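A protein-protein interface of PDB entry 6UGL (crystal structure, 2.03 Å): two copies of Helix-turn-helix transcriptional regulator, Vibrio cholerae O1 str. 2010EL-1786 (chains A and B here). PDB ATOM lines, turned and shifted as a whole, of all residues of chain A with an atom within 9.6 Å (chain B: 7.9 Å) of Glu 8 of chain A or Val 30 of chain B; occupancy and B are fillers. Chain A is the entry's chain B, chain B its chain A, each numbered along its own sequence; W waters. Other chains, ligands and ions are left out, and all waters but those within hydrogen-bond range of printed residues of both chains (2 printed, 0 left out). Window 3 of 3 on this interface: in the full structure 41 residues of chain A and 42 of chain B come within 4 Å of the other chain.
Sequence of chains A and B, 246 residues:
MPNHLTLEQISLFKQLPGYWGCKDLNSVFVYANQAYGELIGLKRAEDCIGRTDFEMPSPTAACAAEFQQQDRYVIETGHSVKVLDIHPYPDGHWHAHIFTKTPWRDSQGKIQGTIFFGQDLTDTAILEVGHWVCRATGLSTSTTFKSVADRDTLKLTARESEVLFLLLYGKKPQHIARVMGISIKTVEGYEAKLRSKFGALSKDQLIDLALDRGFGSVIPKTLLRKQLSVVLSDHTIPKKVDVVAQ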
ATOM      1  N   LEU A   5      -8.409  -3.735  26.634  1.00  0.00           N
ATOM      2  CA  LEU A   5      -8.377  -5.189  26.575  1.00  0.00           C
ATOM      3  C   LEU A   5      -8.912  -5.794  27.864  1.00  0.00           C
ATOM      4  O   LEU A   5      -8.679  -5.278  28.959  1.00  0.00           O
ATOM      5  CB  LEU A   5      -6.965  -5.729  26.336  1.00  0.00           C
ATOM      6  CG  LEU A   5      -6.308  -5.506  24.974  1.00  0.00           C
ATOM      7  CD1 LEU A   5      -4.964  -6.219  24.927  1.00  0.00           C
ATOM      8  CD2 LEU A   5      -7.211  -5.982  23.845  1.00  0.00           C
ATOM      9  N   THR A   6      -9.606  -6.918  27.715  1.00  0.00           N
ATOM     10  CA  THR A   6     -10.082  -7.719  28.829  1.00  0.00           C
ATOM     11  C   THR A   6      -8.934  -8.522  29.442  1.00  0.00           C
ATOM     12  O   THR A   6      -7.861  -8.676  28.854  1.00  0.00           O
ATOM     13  CB  THR A   6     -11.191  -8.671  28.367  1.00  0.00           C
ATOM     14  OG1 THR A   6     -10.633  -9.676  27.513  1.00  0.00           O
ATOM     15  CG2 THR A   6     -12.252  -7.922  27.582  1.00  0.00           C
ATOM     16  N   LEU A   7      -9.181  -9.058  30.639  1.00  0.00           N
ATOM     17  CA  LEU A   7      -8.193  -9.910  31.298  1.00  0.00           C
ATOM     18  C   LEU A   7      -7.823 -11.116  30.439  1.00  0.00           C
ATOM     19  O   LEU A   7      -6.653 -11.507  30.381  1.00  0.00           O
ATOM     20  CB  LEU A   7      -8.719 -10.366  32.662  1.00  0.00           C
ATOM     21  CG  LEU A   7      -8.873  -9.293  33.742  1.00  0.00           C
ATOM     22  CD1 LEU A   7      -9.370  -9.893  35.060  1.00  0.00           C
ATOM     23  CD2 LEU A   7      -7.555  -8.542  33.946  1.00  0.00           C
ATOM     24  N   GLU A   8      -8.804 -11.723  29.756  1.00  0.00           N
ATOM     25  CA  GLU A   8      -8.490 -12.876  28.915  1.00  0.00           C
ATOM     26  C   GLU A   8      -7.679 -12.470  27.691  1.00  0.00           C
ATOM     27  O   GLU A   8      -6.820 -13.233  27.232  1.00  0.00           O
ATOM     28  CB  GLU A   8      -9.772 -13.588  28.475  1.00  0.00           C
ATOM     29  CG  GLU A   8     -10.434 -14.356  29.580  1.00  0.00           C
ATOM     30  CD  GLU A   8     -11.925 -14.189  29.568  1.00  0.00           C
ATOM     31  OE1 GLU A   8     -12.486 -13.886  28.489  1.00  0.00           O
ATOM     32  OE2 GLU A   8     -12.532 -14.356  30.641  1.00  0.00           O
ATOM     33  N   GLN A   9      -7.968 -11.296  27.127  1.00  0.00           N
ATOM     34  CA  GLN A   9      -7.212 -10.820  25.977  1.00  0.00           C
ATOM     35  C   GLN A   9      -5.792 -10.424  26.384  1.00  0.00           C
ATOM     36  O   GLN A   9      -4.836 -10.668  25.639  1.00  0.00           O
ATOM     37  CB  GLN A   9      -7.943  -9.648  25.316  1.00  0.00           C
ATOM     38  CG  GLN A   9      -9.257 -10.023  24.634  1.00  0.00           C
ATOM     39  CD  GLN A   9     -10.217  -8.851  24.485  1.00  0.00           C
ATOM     40  OE1 GLN A   9      -9.853  -7.694  24.687  1.00  0.00           O
ATOM     41  NE2 GLN A   9     -11.460  -9.156  24.133  1.00  0.00           N
ATOM     42  N   ILE A  10      -5.624  -9.851  27.578  1.00  0.00           N
ATOM     43  CA  ILE A  10      -4.268  -9.546  28.050  1.00  0.00           C
ATOM     44  C   ILE A  10      -3.488 -10.839  28.269  1.00  0.00           C
ATOM     45  O   ILE A  10      -2.343 -10.972  27.828  1.00  0.00           O
ATOM     46  CB  ILE A  10      -4.313  -8.673  29.318  1.00  0.00           C
ATOM     47  CG1 ILE A  10      -5.060  -7.373  29.029  1.00  0.00           C
ATOM     48  CG2 ILE A  10      -2.893  -8.321  29.786  1.00  0.00           C
ATOM     49  CD1 ILE A  10      -5.115  -6.413  30.205  1.00  0.00           C
ATOM     50  N   SER A  11      -4.113 -11.828  28.909  1.00  0.00           N
ATOM     51  CA  SER A  11      -3.468 -13.124  29.115  1.00  0.00           C
ATOM     52  C   SER A  11      -3.054 -13.782  27.797  1.00  0.00           C
ATOM     53  O   SER A  11      -1.941 -14.316  27.676  1.00  0.00           O
ATOM     54  CB  SER A  11      -4.402 -14.051  29.886  1.00  0.00           C
ATOM     55  OG  SER A  11      -3.878 -15.361  29.882  1.00  0.00           O
ATOM     56  N   LEU A  12      -3.945 -13.788  26.804  1.00  0.00           N
ATOM     57  CA  LEU A  12      -3.585 -14.360  25.510  1.00  0.00           C
ATOM     58  C   LEU A  12      -2.429 -13.593  24.873  1.00  0.00           C
ATOM     59  O   LEU A  12      -1.471 -14.196  24.365  1.00  0.00           O
ATOM     60  CB  LEU A  12      -4.798 -14.369  24.585  1.00  0.00           C
ATOM     61  CG  LEU A  12      -4.493 -14.680  23.119  1.00  0.00           C
ATOM     62  CD1 LEU A  12      -4.016 -16.110  22.987  1.00  0.00           C
ATOM     63  CD2 LEU A  12      -5.719 -14.408  22.251  1.00  0.00           C
ATOM     64  N   PHE A  13      -2.493 -12.259  24.916  1.00  0.00           N
ATOM     65  CA  PHE A  13      -1.443 -11.434  24.340  1.00  0.00           C
ATOM     66  C   PHE A  13      -0.077 -11.802  24.896  1.00  0.00           C
ATOM     67  O   PHE A  13       0.919 -11.764  24.166  1.00  0.00           O
ATOM     68  CB  PHE A  13      -1.752  -9.964  24.601  1.00  0.00           C
ATOM     69  CG  PHE A  13      -0.882  -9.010  23.842  1.00  0.00           C
ATOM     70  CD1 PHE A  13      -0.703  -9.144  22.482  1.00  0.00           C
ATOM     71  CD2 PHE A  13      -0.272  -7.952  24.485  1.00  0.00           C
ATOM     72  CE1 PHE A  13       0.083  -8.248  21.784  1.00  0.00           C
ATOM     73  CE2 PHE A  13       0.518  -7.061  23.789  1.00  0.00           C
ATOM     74  CZ  PHE A  13       0.692  -7.209  22.435  1.00  0.00           C
ATOM     75  N   LYS A  14      -0.022 -12.209  26.168  1.00  0.00           N
ATOM     76  CA  LYS A  14       1.235 -12.526  26.836  1.00  0.00           C
ATOM     77  C   LYS A  14       1.710 -13.946  26.559  1.00  0.00           C
ATOM     78  O   LYS A  14       2.870 -14.256  26.820  1.00  0.00           O
ATOM     79  CB  LYS A  14       1.093 -12.327  28.351  1.00  0.00           C
ATOM     80  CG  LYS A  14       0.767 -10.897  28.791  1.00  0.00           C
ATOM     81  CD  LYS A  14       1.844  -9.924  28.341  1.00  0.00           C
ATOM     82  CE  LYS A  14       1.663  -8.544  28.967  1.00  0.00           C
ATOM     83  NZ  LYS A  14       2.792  -7.630  28.607  1.00  0.00           N
ATOM     84  N   GLN A  15       0.848 -14.818  26.034  1.00  0.00           N
ATOM     85  CA  GLN A  15       1.229 -16.203  25.792  1.00  0.00           C
ATOM     86  C   GLN A  15       1.321 -16.580  24.314  1.00  0.00           C
ATOM     87  O   GLN A  15       1.719 -17.710  24.019  1.00  0.00           O
ATOM     88  CB  GLN A  15       0.253 -17.149  26.516  1.00  0.00           C
ATOM     89  CG  GLN A  15       0.321 -16.945  28.023  1.00  0.00           C
ATOM     90  CD  GLN A  15      -0.703 -17.756  28.769  1.00  0.00           C
ATOM     91  OE1 GLN A  15      -0.710 -18.991  28.701  1.00  0.00           O
ATOM     92  NE2 GLN A  15      -1.590 -17.068  29.490  1.00  0.00           N
ATOM     93  N   LEU A  16       0.974 -15.683  23.390  1.00  0.00           N
ATOM     94  CA  LEU A  16       1.016 -16.011  21.969  1.00  0.00           C
ATOM     95  C   LEU A  16       2.412 -16.512  21.602  1.00  0.00           C
ATOM     96  O   LEU A  16       3.401 -15.945  22.060  1.00  0.00           O
ATOM     97  CB  LEU A  16       0.676 -14.784  21.117  1.00  0.00           C
ATOM     98  CG  LEU A  16      -0.762 -14.270  21.049  1.00  0.00           C
ATOM     99  CD1 LEU A  16      -0.785 -12.911  20.376  1.00  0.00           C
ATOM    100  CD2 LEU A  16      -1.621 -15.230  20.280  1.00  0.00           C
ATOM    101  N   PHE B  13      -1.243  -5.633  19.321  1.00  0.00           N
ATOM    102  CA  PHE B  13      -2.221  -6.693  19.544  1.00  0.00           C
ATOM    103  C   PHE B  13      -3.162  -6.813  18.355  1.00  0.00           C
ATOM    104  O   PHE B  13      -3.445  -7.921  17.888  1.00  0.00           O
ATOM    105  CB  PHE B  13      -3.000  -6.426  20.835  1.00  0.00           C
ATOM    106  CG  PHE B  13      -4.101  -7.429  21.122  1.00  0.00           C
ATOM    107  CD1 PHE B  13      -3.829  -8.605  21.799  1.00  0.00           C
ATOM    108  CD2 PHE B  13      -5.407  -7.178  20.744  1.00  0.00           C
ATOM    109  CE1 PHE B  13      -4.820  -9.513  22.078  1.00  0.00           C
ATOM    110  CE2 PHE B  13      -6.410  -8.090  21.028  1.00  0.00           C
ATOM    111  CZ  PHE B  13      -6.111  -9.259  21.692  1.00  0.00           C
ATOM    112  N   GLY B  21      -5.980 -16.686  18.130  1.00  0.00           N
ATOM    113  CA  GLY B  21      -7.010 -16.631  19.147  1.00  0.00           C
ATOM    114  C   GLY B  21      -6.817 -17.743  20.164  1.00  0.00           C
ATOM    115  O   GLY B  21      -5.774 -18.404  20.198  1.00  0.00           O
ATOM    116  N   CYS B  22      -7.860 -17.950  20.976  1.00  0.00           N
ATOM    117  CA  CYS B  22      -7.833 -18.965  22.024  1.00  0.00           C
ATOM    118  C   CYS B  22      -9.238 -19.479  22.312  1.00  0.00           C
ATOM    119  O   CYS B  22     -10.228 -18.763  22.135  1.00  0.00           O
ATOM    120  CB  CYS B  22      -7.218 -18.431  23.328  1.00  0.00           C
ATOM    121  SG  CYS B  22      -8.079 -17.008  24.083  1.00  0.00           S
ATOM    122  N   LYS B  23      -9.301 -20.722  22.793  1.00  0.00           N
ATOM    123  CA  LYS B  23     -10.536 -21.386  23.175  1.00  0.00           C
ATOM    124  C   LYS B  23     -10.365 -21.927  24.586  1.00  0.00           C
ATOM    125  O   LYS B  23      -9.242 -22.086  25.060  1.00  0.00           O
ATOM    126  CB  LYS B  23     -10.887 -22.548  22.220  1.00  0.00           C
ATOM    127  CG  LYS B  23     -10.652 -22.288  20.745  1.00  0.00           C
ATOM    128  CD  LYS B  23     -10.592 -23.638  19.988  1.00  0.00           C
ATOM    129  CE  LYS B  23     -10.085 -23.516  18.552  1.00  0.00           C
ATOM    130  NZ  LYS B  23     -10.109 -24.841  17.826  1.00  0.00           N
ATOM    131  N   ASP B  24     -11.482 -22.248  25.243  1.00  0.00           N
ATOM    132  CA  ASP B  24     -11.435 -22.810  26.585  1.00  0.00           C
ATOM    133  C   ASP B  24     -11.291 -24.332  26.533  1.00  0.00           C
ATOM    134  O   ASP B  24     -10.998 -24.916  25.488  1.00  0.00           O
ATOM    135  CB  ASP B  24     -12.638 -22.355  27.413  1.00  0.00           C
ATOM    136  CG  ASP B  24     -13.993 -22.894  26.900  1.00  0.00           C
ATOM    137  OD1 ASP B  24     -14.061 -23.811  26.049  1.00  0.00           O
ATOM    138  OD2 ASP B  24     -15.015 -22.372  27.399  1.00  0.00           O
ATOM    139  N   LEU B  25     -11.485 -24.986  27.679  1.00  0.00           N
ATOM    140  CA  LEU B  25     -11.258 -26.425  27.796  1.00  0.00           C
ATOM    141  C   LEU B  25     -12.244 -27.256  26.963  1.00  0.00           C
ATOM    142  O   LEU B  25     -11.952 -28.419  26.655  1.00  0.00           O
ATOM    143  CB  LEU B  25     -11.319 -26.821  29.279  1.00  0.00           C
ATOM    144  CG  LEU B  25     -10.166 -26.227  30.126  1.00  0.00           C
ATOM    145  CD1 LEU B  25     -10.342 -26.460  31.618  1.00  0.00           C
ATOM    146  CD2 LEU B  25      -8.829 -26.785  29.655  1.00  0.00           C
ATOM    147  N   SER B  27     -13.007 -26.225  23.948  1.00  0.00           N
ATOM    148  CA  SER B  27     -12.755 -25.639  22.626  1.00  0.00           C
ATOM    149  C   SER B  27     -13.891 -24.710  22.199  1.00  0.00           C
ATOM    150  O   SER B  27     -14.295 -24.681  21.031  1.00  0.00           O
ATOM    151  CB  SER B  27     -12.516 -26.719  21.572  1.00  0.00           C
ATOM    152  OG  SER B  27     -11.382 -27.493  21.905  1.00  0.00           O
ATOM    153  N   VAL B  28     -14.417 -23.954  23.162  1.00  0.00           N
ATOM    154  CA  VAL B  28     -15.334 -22.855  22.882  1.00  0.00           C
ATOM    155  C   VAL B  28     -14.508 -21.585  22.753  1.00  0.00           C
ATOM    156  O   VAL B  28     -13.681 -21.292  23.621  1.00  0.00           O
ATOM    157  CB  VAL B  28     -16.387 -22.719  23.992  1.00  0.00           C
ATOM    158  CG1 VAL B  28     -17.075 -21.367  23.903  1.00  0.00           C
ATOM    159  CG2 VAL B  28     -17.412 -23.856  23.895  1.00  0.00           C
ATOM    160  N   PHE B  29     -14.732 -20.831  21.677  1.00  0.00           N
ATOM    161  CA  PHE B  29     -13.900 -19.669  21.387  1.00  0.00           C
ATOM    162  C   PHE B  29     -14.008 -18.611  22.489  1.00  0.00           C
ATOM    163  O   PHE B  29     -15.106 -18.243  22.919  1.00  0.00           O
ATOM    164  CB  PHE B  29     -14.293 -19.064  20.035  1.00  0.00           C
ATOM    165  CG  PHE B  29     -13.604 -19.703  18.849  1.00  0.00           C
ATOM    166  CD1 PHE B  29     -13.782 -21.046  18.563  1.00  0.00           C
ATOM    167  CD2 PHE B  29     -12.777 -18.953  18.023  1.00  0.00           C
ATOM    168  CE1 PHE B  29     -13.150 -21.631  17.476  1.00  0.00           C
ATOM    169  CE2 PHE B  29     -12.137 -19.535  16.931  1.00  0.00           C
ATOM    170  CZ  PHE B  29     -12.316 -20.873  16.665  1.00  0.00           C
ATOM    171  N   VAL B  30     -12.854 -18.115  22.921  1.00  0.00           N
ATOM    172  CA  VAL B  30     -12.763 -17.021  23.876  1.00  0.00           C
ATOM    173  C   VAL B  30     -12.302 -15.734  23.204  1.00  0.00           C
ATOM    174  O   VAL B  30     -12.811 -14.656  23.511  1.00  0.00           O
ATOM    175  CB  VAL B  30     -11.838 -17.398  25.057  1.00  0.00           C
ATOM    176  CG1 VAL B  30     -11.555 -16.179  25.980  1.00  0.00           C
ATOM    177  CG2 VAL B  30     -12.474 -18.526  25.861  1.00  0.00           C
ATOM    178  N   TYR B  31     -11.392 -15.835  22.240  1.00  0.00           N
ATOM    179  CA  TYR B  31     -11.024 -14.683  21.439  1.00  0.00           C
ATOM    180  C   TYR B  31     -10.563 -15.161  20.069  1.00  0.00           C
ATOM    181  O   TYR B  31      -9.992 -16.246  19.936  1.00  0.00           O
ATOM    182  CB  TYR B  31      -9.912 -13.849  22.104  1.00  0.00           C
ATOM    183  CG  TYR B  31      -9.557 -12.634  21.286  1.00  0.00           C
ATOM    184  CD1 TYR B  31     -10.330 -11.469  21.363  1.00  0.00           C
ATOM    185  CD2 TYR B  31      -8.469 -12.650  20.425  1.00  0.00           C
ATOM    186  CE1 TYR B  31     -10.025 -10.370  20.593  1.00  0.00           C
ATOM    187  CE2 TYR B  31      -8.160 -11.560  19.650  1.00  0.00           C
ATOM    188  CZ  TYR B  31      -8.931 -10.420  19.743  1.00  0.00           C
ATOM    189  OH  TYR B  31      -8.611  -9.336  18.969  1.00  0.00           O
ATOM    190  N   ALA B  32     -10.826 -14.349  19.051  1.00  0.00           N
ATOM    191  CA  ALA B  32     -10.208 -14.536  17.739  1.00  0.00           C
ATOM    192  C   ALA B  32      -9.865 -13.173  17.170  1.00  0.00           C
ATOM    193  O   ALA B  32     -10.669 -12.240  17.270  1.00  0.00           O
ATOM    194  CB  ALA B  32     -11.130 -15.293  16.761  1.00  0.00           C
ATOM    195  N   ALA B  45     -15.092 -10.286  14.216  1.00  0.00           N
ATOM    196  CA  ALA B  45     -14.516 -11.464  14.850  1.00  0.00           C
ATOM    197  C   ALA B  45     -15.083 -11.709  16.241  1.00  0.00           C
ATOM    198  O   ALA B  45     -14.923 -12.816  16.770  1.00  0.00           O
ATOM    199  CB  ALA B  45     -12.981 -11.340  14.915  1.00  0.00           C
ATOM    200  N   GLU B  46     -15.756 -10.710  16.828  1.00  0.00           N
ATOM    201  CA  GLU B  46     -16.430 -10.901  18.110  1.00  0.00           C
ATOM    202  C   GLU B  46     -17.504 -11.980  18.049  1.00  0.00           C
ATOM    203  O   GLU B  46     -17.853 -12.561  19.082  1.00  0.00           O
ATOM    204  CB  GLU B  46     -17.080  -9.594  18.580  1.00  0.00           C
ATOM    205  CG  GLU B  46     -16.117  -8.491  18.948  1.00  0.00           C
ATOM    206  CD  GLU B  46     -15.708  -7.637  17.758  1.00  0.00           C
ATOM    207  OE1 GLU B  46     -15.971  -8.020  16.593  1.00  0.00           O
ATOM    208  OE2 GLU B  46     -15.127  -6.565  17.993  1.00  0.00           O
ATOM    209  N   CYS B  48     -17.240 -14.865  16.941  1.00  0.00           N
ATOM    210  CA  CYS B  48     -16.681 -16.182  17.241  1.00  0.00           C
ATOM    211  C   CYS B  48     -16.896 -16.560  18.700  1.00  0.00           C
ATOM    212  O   CYS B  48     -17.052 -17.743  19.027  1.00  0.00           O
ATOM    213  CB  CYS B  48     -15.182 -16.200  16.940  1.00  0.00           C
ATOM    214  SG  CYS B  48     -14.790 -15.974  15.203  1.00  0.00           S
ATOM    215  N   ILE B  49     -16.883 -15.564  19.585  1.00  0.00           N
ATOM    216  CA  ILE B  49     -16.838 -15.820  21.018  1.00  0.00           C
ATOM    217  C   ILE B  49     -18.100 -16.548  21.462  1.00  0.00           C
ATOM    218  O   ILE B  49     -19.225 -16.146  21.134  1.00  0.00           O
ATOM    219  CB  ILE B  49     -16.627 -14.495  21.768  1.00  0.00           C
ATOM    220  CG1 ILE B  49     -15.331 -13.830  21.281  1.00  0.00           C
ATOM    221  CG2 ILE B  49     -16.576 -14.729  23.266  1.00  0.00           C
ATOM    222  CD1 ILE B  49     -15.217 -12.348  21.583  1.00  0.00           C
ATOM    223  N   GLY B  50     -17.913 -17.632  22.215  1.00  0.00           N
ATOM    224  CA  GLY B  50     -19.009 -18.430  22.714  1.00  0.00           C
ATOM    225  C   GLY B  50     -19.400 -19.583  21.814  1.00  0.00           C
ATOM    226  O   GLY B  50     -20.193 -20.432  22.228  1.00  0.00           O
ATOM    227  N   ARG B  51     -18.870 -19.644  20.607  1.00  0.00           N
ATOM    228  CA  ARG B  51     -19.224 -20.702  19.677  1.00  0.00           C
ATOM    229  C   ARG B  51     -18.085 -21.702  19.535  1.00  0.00           C
ATOM    230  O   ARG B  51     -16.923 -21.418  19.853  1.00  0.00           O
ATOM    231  CB  ARG B  51     -19.608 -20.106  18.320  1.00  0.00           C
ATOM    232  CG  ARG B  51     -20.914 -19.309  18.391  1.00  0.00           C
ATOM    233  CD  ARG B  51     -21.020 -18.239  17.315  1.00  0.00           C
ATOM    234  NE  ARG B  51     -21.287 -18.784  15.985  1.00  0.00           N
ATOM    235  CZ  ARG B  51     -21.767 -18.070  14.969  1.00  0.00           C
ATOM    236  NH1 ARG B  51     -22.039 -16.782  15.129  1.00  0.00           N
ATOM    237  NH2 ARG B  51     -21.986 -18.640  13.794  1.00  0.00           N
ATOM    238  N   TRP B 104      -3.108 -22.847  26.751  1.00  0.00           N
ATOM    239  CA  TRP B 104      -3.398 -21.536  27.319  1.00  0.00           C
ATOM    240  C   TRP B 104      -3.466 -21.682  28.839  1.00  0.00           C
ATOM    241  O   TRP B 104      -4.282 -22.458  29.351  1.00  0.00           O
ATOM    242  CB  TRP B 104      -4.710 -20.983  26.758  1.00  0.00           C
ATOM    243  CG  TRP B 104      -5.055 -19.616  27.275  1.00  0.00           C
ATOM    244  CD1 TRP B 104      -4.179 -18.657  27.711  1.00  0.00           C
ATOM    245  CD2 TRP B 104      -6.368 -19.061  27.431  1.00  0.00           C
ATOM    246  NE1 TRP B 104      -4.866 -17.538  28.110  1.00  0.00           N
ATOM    247  CE2 TRP B 104      -6.210 -17.760  27.968  1.00  0.00           C
ATOM    248  CE3 TRP B 104      -7.656 -19.535  27.186  1.00  0.00           C
ATOM    249  CZ2 TRP B 104      -7.291 -16.928  28.240  1.00  0.00           C
ATOM    250  CZ3 TRP B 104      -8.736 -18.704  27.464  1.00  0.00           C
ATOM    251  CH2 TRP B 104      -8.543 -17.415  27.988  1.00  0.00           C
ATOM    252  N   ARG B 105      -2.604 -20.957  29.552  1.00  0.00           N
ATOM    253  CA  ARG B 105      -2.465 -21.089  30.997  1.00  0.00           C
ATOM    254  C   ARG B 105      -3.001 -19.856  31.715  1.00  0.00           C
ATOM    255  O   ARG B 105      -2.994 -18.748  31.173  1.00  0.00           O
ATOM    256  CB  ARG B 105      -1.003 -21.331  31.387  1.00  0.00           C
ATOM    257  CG  ARG B 105      -0.552 -22.739  31.060  1.00  0.00           C
ATOM    258  CD  ARG B 105       0.948 -22.963  31.206  1.00  0.00           C
ATOM    259  NE  ARG B 105       1.206 -24.399  31.266  1.00  0.00           N
ATOM    260  CZ  ARG B 105       1.742 -25.114  30.285  1.00  0.00           C
ATOM    261  NH1 ARG B 105       2.111 -24.528  29.148  1.00  0.00           N
ATOM    262  NH2 ARG B 105       1.922 -26.418  30.447  1.00  0.00           N
ATOM    263  N   GLN B 112      -6.014 -23.767  30.925  1.00  0.00           N
ATOM    264  CA  GLN B 112      -7.410 -23.345  30.880  1.00  0.00           C
ATOM    265  C   GLN B 112      -7.983 -23.364  29.467  1.00  0.00           C
ATOM    266  O   GLN B 112      -9.146 -22.975  29.265  1.00  0.00           O
ATOM    267  CB  GLN B 112      -7.566 -21.938  31.476  1.00  0.00           C
ATOM    268  CG  GLN B 112      -6.809 -20.835  30.731  1.00  0.00           C
ATOM    269  CD  GLN B 112      -6.941 -19.488  31.442  1.00  0.00           C
ATOM    270  OE1 GLN B 112      -7.877 -19.282  32.211  1.00  0.00           O
ATOM    271  NE2 GLN B 112      -6.002 -18.577  31.196  1.00  0.00           N
ATOM    272  N   GLY B 113      -7.212 -23.824  28.495  1.00  0.00           N
ATOM    273  CA  GLY B 113      -7.659 -23.901  27.117  1.00  0.00           C
ATOM    274  C   GLY B 113      -6.461 -24.019  26.195  1.00  0.00           C
ATOM    275  O   GLY B 113      -5.395 -24.489  26.599  1.00  0.00           O
ATOM    276  N   THR B 114      -6.662 -23.583  24.957  1.00  0.00           N
ATOM    277  CA  THR B 114      -5.615 -23.648  23.956  1.00  0.00           C
ATOM    278  C   THR B 114      -5.497 -22.304  23.271  1.00  0.00           C
ATOM    279  O   THR B 114      -6.443 -21.514  23.223  1.00  0.00           O
ATOM    280  CB  THR B 114      -5.875 -24.720  22.870  1.00  0.00           C
ATOM    281  OG1 THR B 114      -7.109 -24.437  22.218  1.00  0.00           O
ATOM    282  CG2 THR B 114      -5.877 -26.126  23.454  1.00  0.00           C
ATOM    283  N   PHE B 116      -4.311 -20.909  19.435  1.00  0.00           N
ATOM    284  CA  PHE B 116      -4.045 -21.301  18.056  1.00  0.00           C
ATOM    285  C   PHE B 116      -3.440 -20.126  17.306  1.00  0.00           C
ATOM    286  O   PHE B 116      -3.807 -18.974  17.540  1.00  0.00           O
ATOM    287  CB  PHE B 116      -5.311 -21.811  17.324  1.00  0.00           C
ATOM    288  CG  PHE B 116      -6.448 -20.816  17.276  1.00  0.00           C
ATOM    289  CD1 PHE B 116      -7.395 -20.790  18.291  1.00  0.00           C
ATOM    290  CD2 PHE B 116      -6.581 -19.925  16.211  1.00  0.00           C
ATOM    291  CE1 PHE B 116      -8.457 -19.879  18.268  1.00  0.00           C
ATOM    292  CE2 PHE B 116      -7.639 -19.002  16.182  1.00  0.00           C
ATOM    293  CZ  PHE B 116      -8.581 -18.991  17.205  1.00  0.00           C
HETATM  294  O   HOH W   1     -12.506 -11.876  23.976  1.00  0.00           O
HETATM  295  O   HOH W   2     -14.086 -14.148  26.002  1.00  0.00           O
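Glu 8 of chain A touches just these residues of chain B: Val 30 (3.5 Å) and Trp 104 (3.9 Å).
Of the printed residues of chain B, Ser 11 of chain A touches Trp 104 (3.0 Å) and Arg 105 (3.7 Å).
Of the printed residues of chain A, Phe 13 of chain B touches Leu 5, Gln 9 and Phe 13.
Of chain A, only Leu 12 comes within 4 Å of Cys 22 of chain B.
Ser 27 of chain B touches none of the printed residues of chain A.
Val 30 of chain B touches one residue of chain A.
Ile 49 of chain B touches none of the printed residues of chain A.
Of the printed residues of chain A, Arg 105 of chain B touches Ser 11 (3.7 Å) and Gln 15 (2.8 Å).
The nearest residue of chain B that does not touch Glu 8 of chain A is Cys 22 of chain B (5.1 Å).
The nearest residue of chain A that does not touch Val 30 of chain B is Gln 9 of chain A (5.7 Å).
The indole nitrogen (NE1) of Trp 104 of chain B sits at hydrogen-bond distance from the side-chain hydroxyl (OG) of Ser 11 of chain A, at 3.0 Å.
The backbone carbonyl oxygen (O) of Arg 105 of chain B sits at hydrogen-bond distance from the side-chain amide nitrogen (NE2) of Gln 15 of chain A, at 2.8 Å.
Phe 13 of chain A touches its own counterpart, Phe 13 of chain B.
Position printed for both chains: 13.
Of the 12 pairs that touch across the chains among the printed residues, 1 has its exchanged pair printed and touching as well.
Among the printed residues, pairs that only touch across the chains: Phe 13 of chain A with Phe 13 of chain B (3.2 Å), Gln 15 of chain A with Trp 104 of chain B (3.5 Å), Glu 8 of chain A with Val 30 of chain B (3.5 Å), Leu 5 of chain A with Phe 13 of chain B (3.6 Å), Ser 11 of chain A with Arg 105 of chain B (3.7 Å), Gln 9 of chain A with Tyr 31 of chain B (3.7 Å), Leu 12 of chain A with Tyr 31 of chain B (3.7 Å), Gln 9 of chain A with Phe 13 of chain B (3.7 Å), Glu 8 of chain A with Trp 104 of chain B (3.9 Å) and Leu 12 of chain A with Cys 22 of chain B (3.96 Å).
O of Cys 22 of chain B sits at hydrogen-bond distance from N of Val 30 of chain B (2.8 Å).
O of Arg 105 of chain B lies within hydrogen-bond range of NE2 of Gln 112 of chain B (3.0 Å).
OE1 of Gln 9 of chain A lies within hydrogen-bond range of N of Thr 6 of chain A (3.1 Å).
OG of Ser 11 of chain A is in hydrogen-bond range of NE2 of Gln 15 of chain A, 2.9 Å away.
The backbone carbonyl oxygen (O) of Trp 104 of chain B lies within hydrogen-bond range of the backbone NH (N) of Gln 112 of chain B (2.7 Å).
O of Tyr 31 of chain B lies within hydrogen-bond range of N of Cys 22 of chain B (2.9 Å).
Among the printed residues, no Asp or Glu carboxylate lies within 4 Å of a Lys or Arg side-chain nitrogen of the other chain.
Water W1 lies within hydrogen-bond range of the backbone carbonyl oxygen (O) of Val 30 of chain B (2.8 Å) and the side-chain amide nitrogen (NE2) of Gln 9 of chain A (2.9 Å).
Water W2 lies within hydrogen-bond range of the backbone carbonyl oxygen (O) of Val 30 of chain B (2.8 Å) and the side-chain carboxylate (OE1) of Glu 8 of chain A (3.0 Å).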
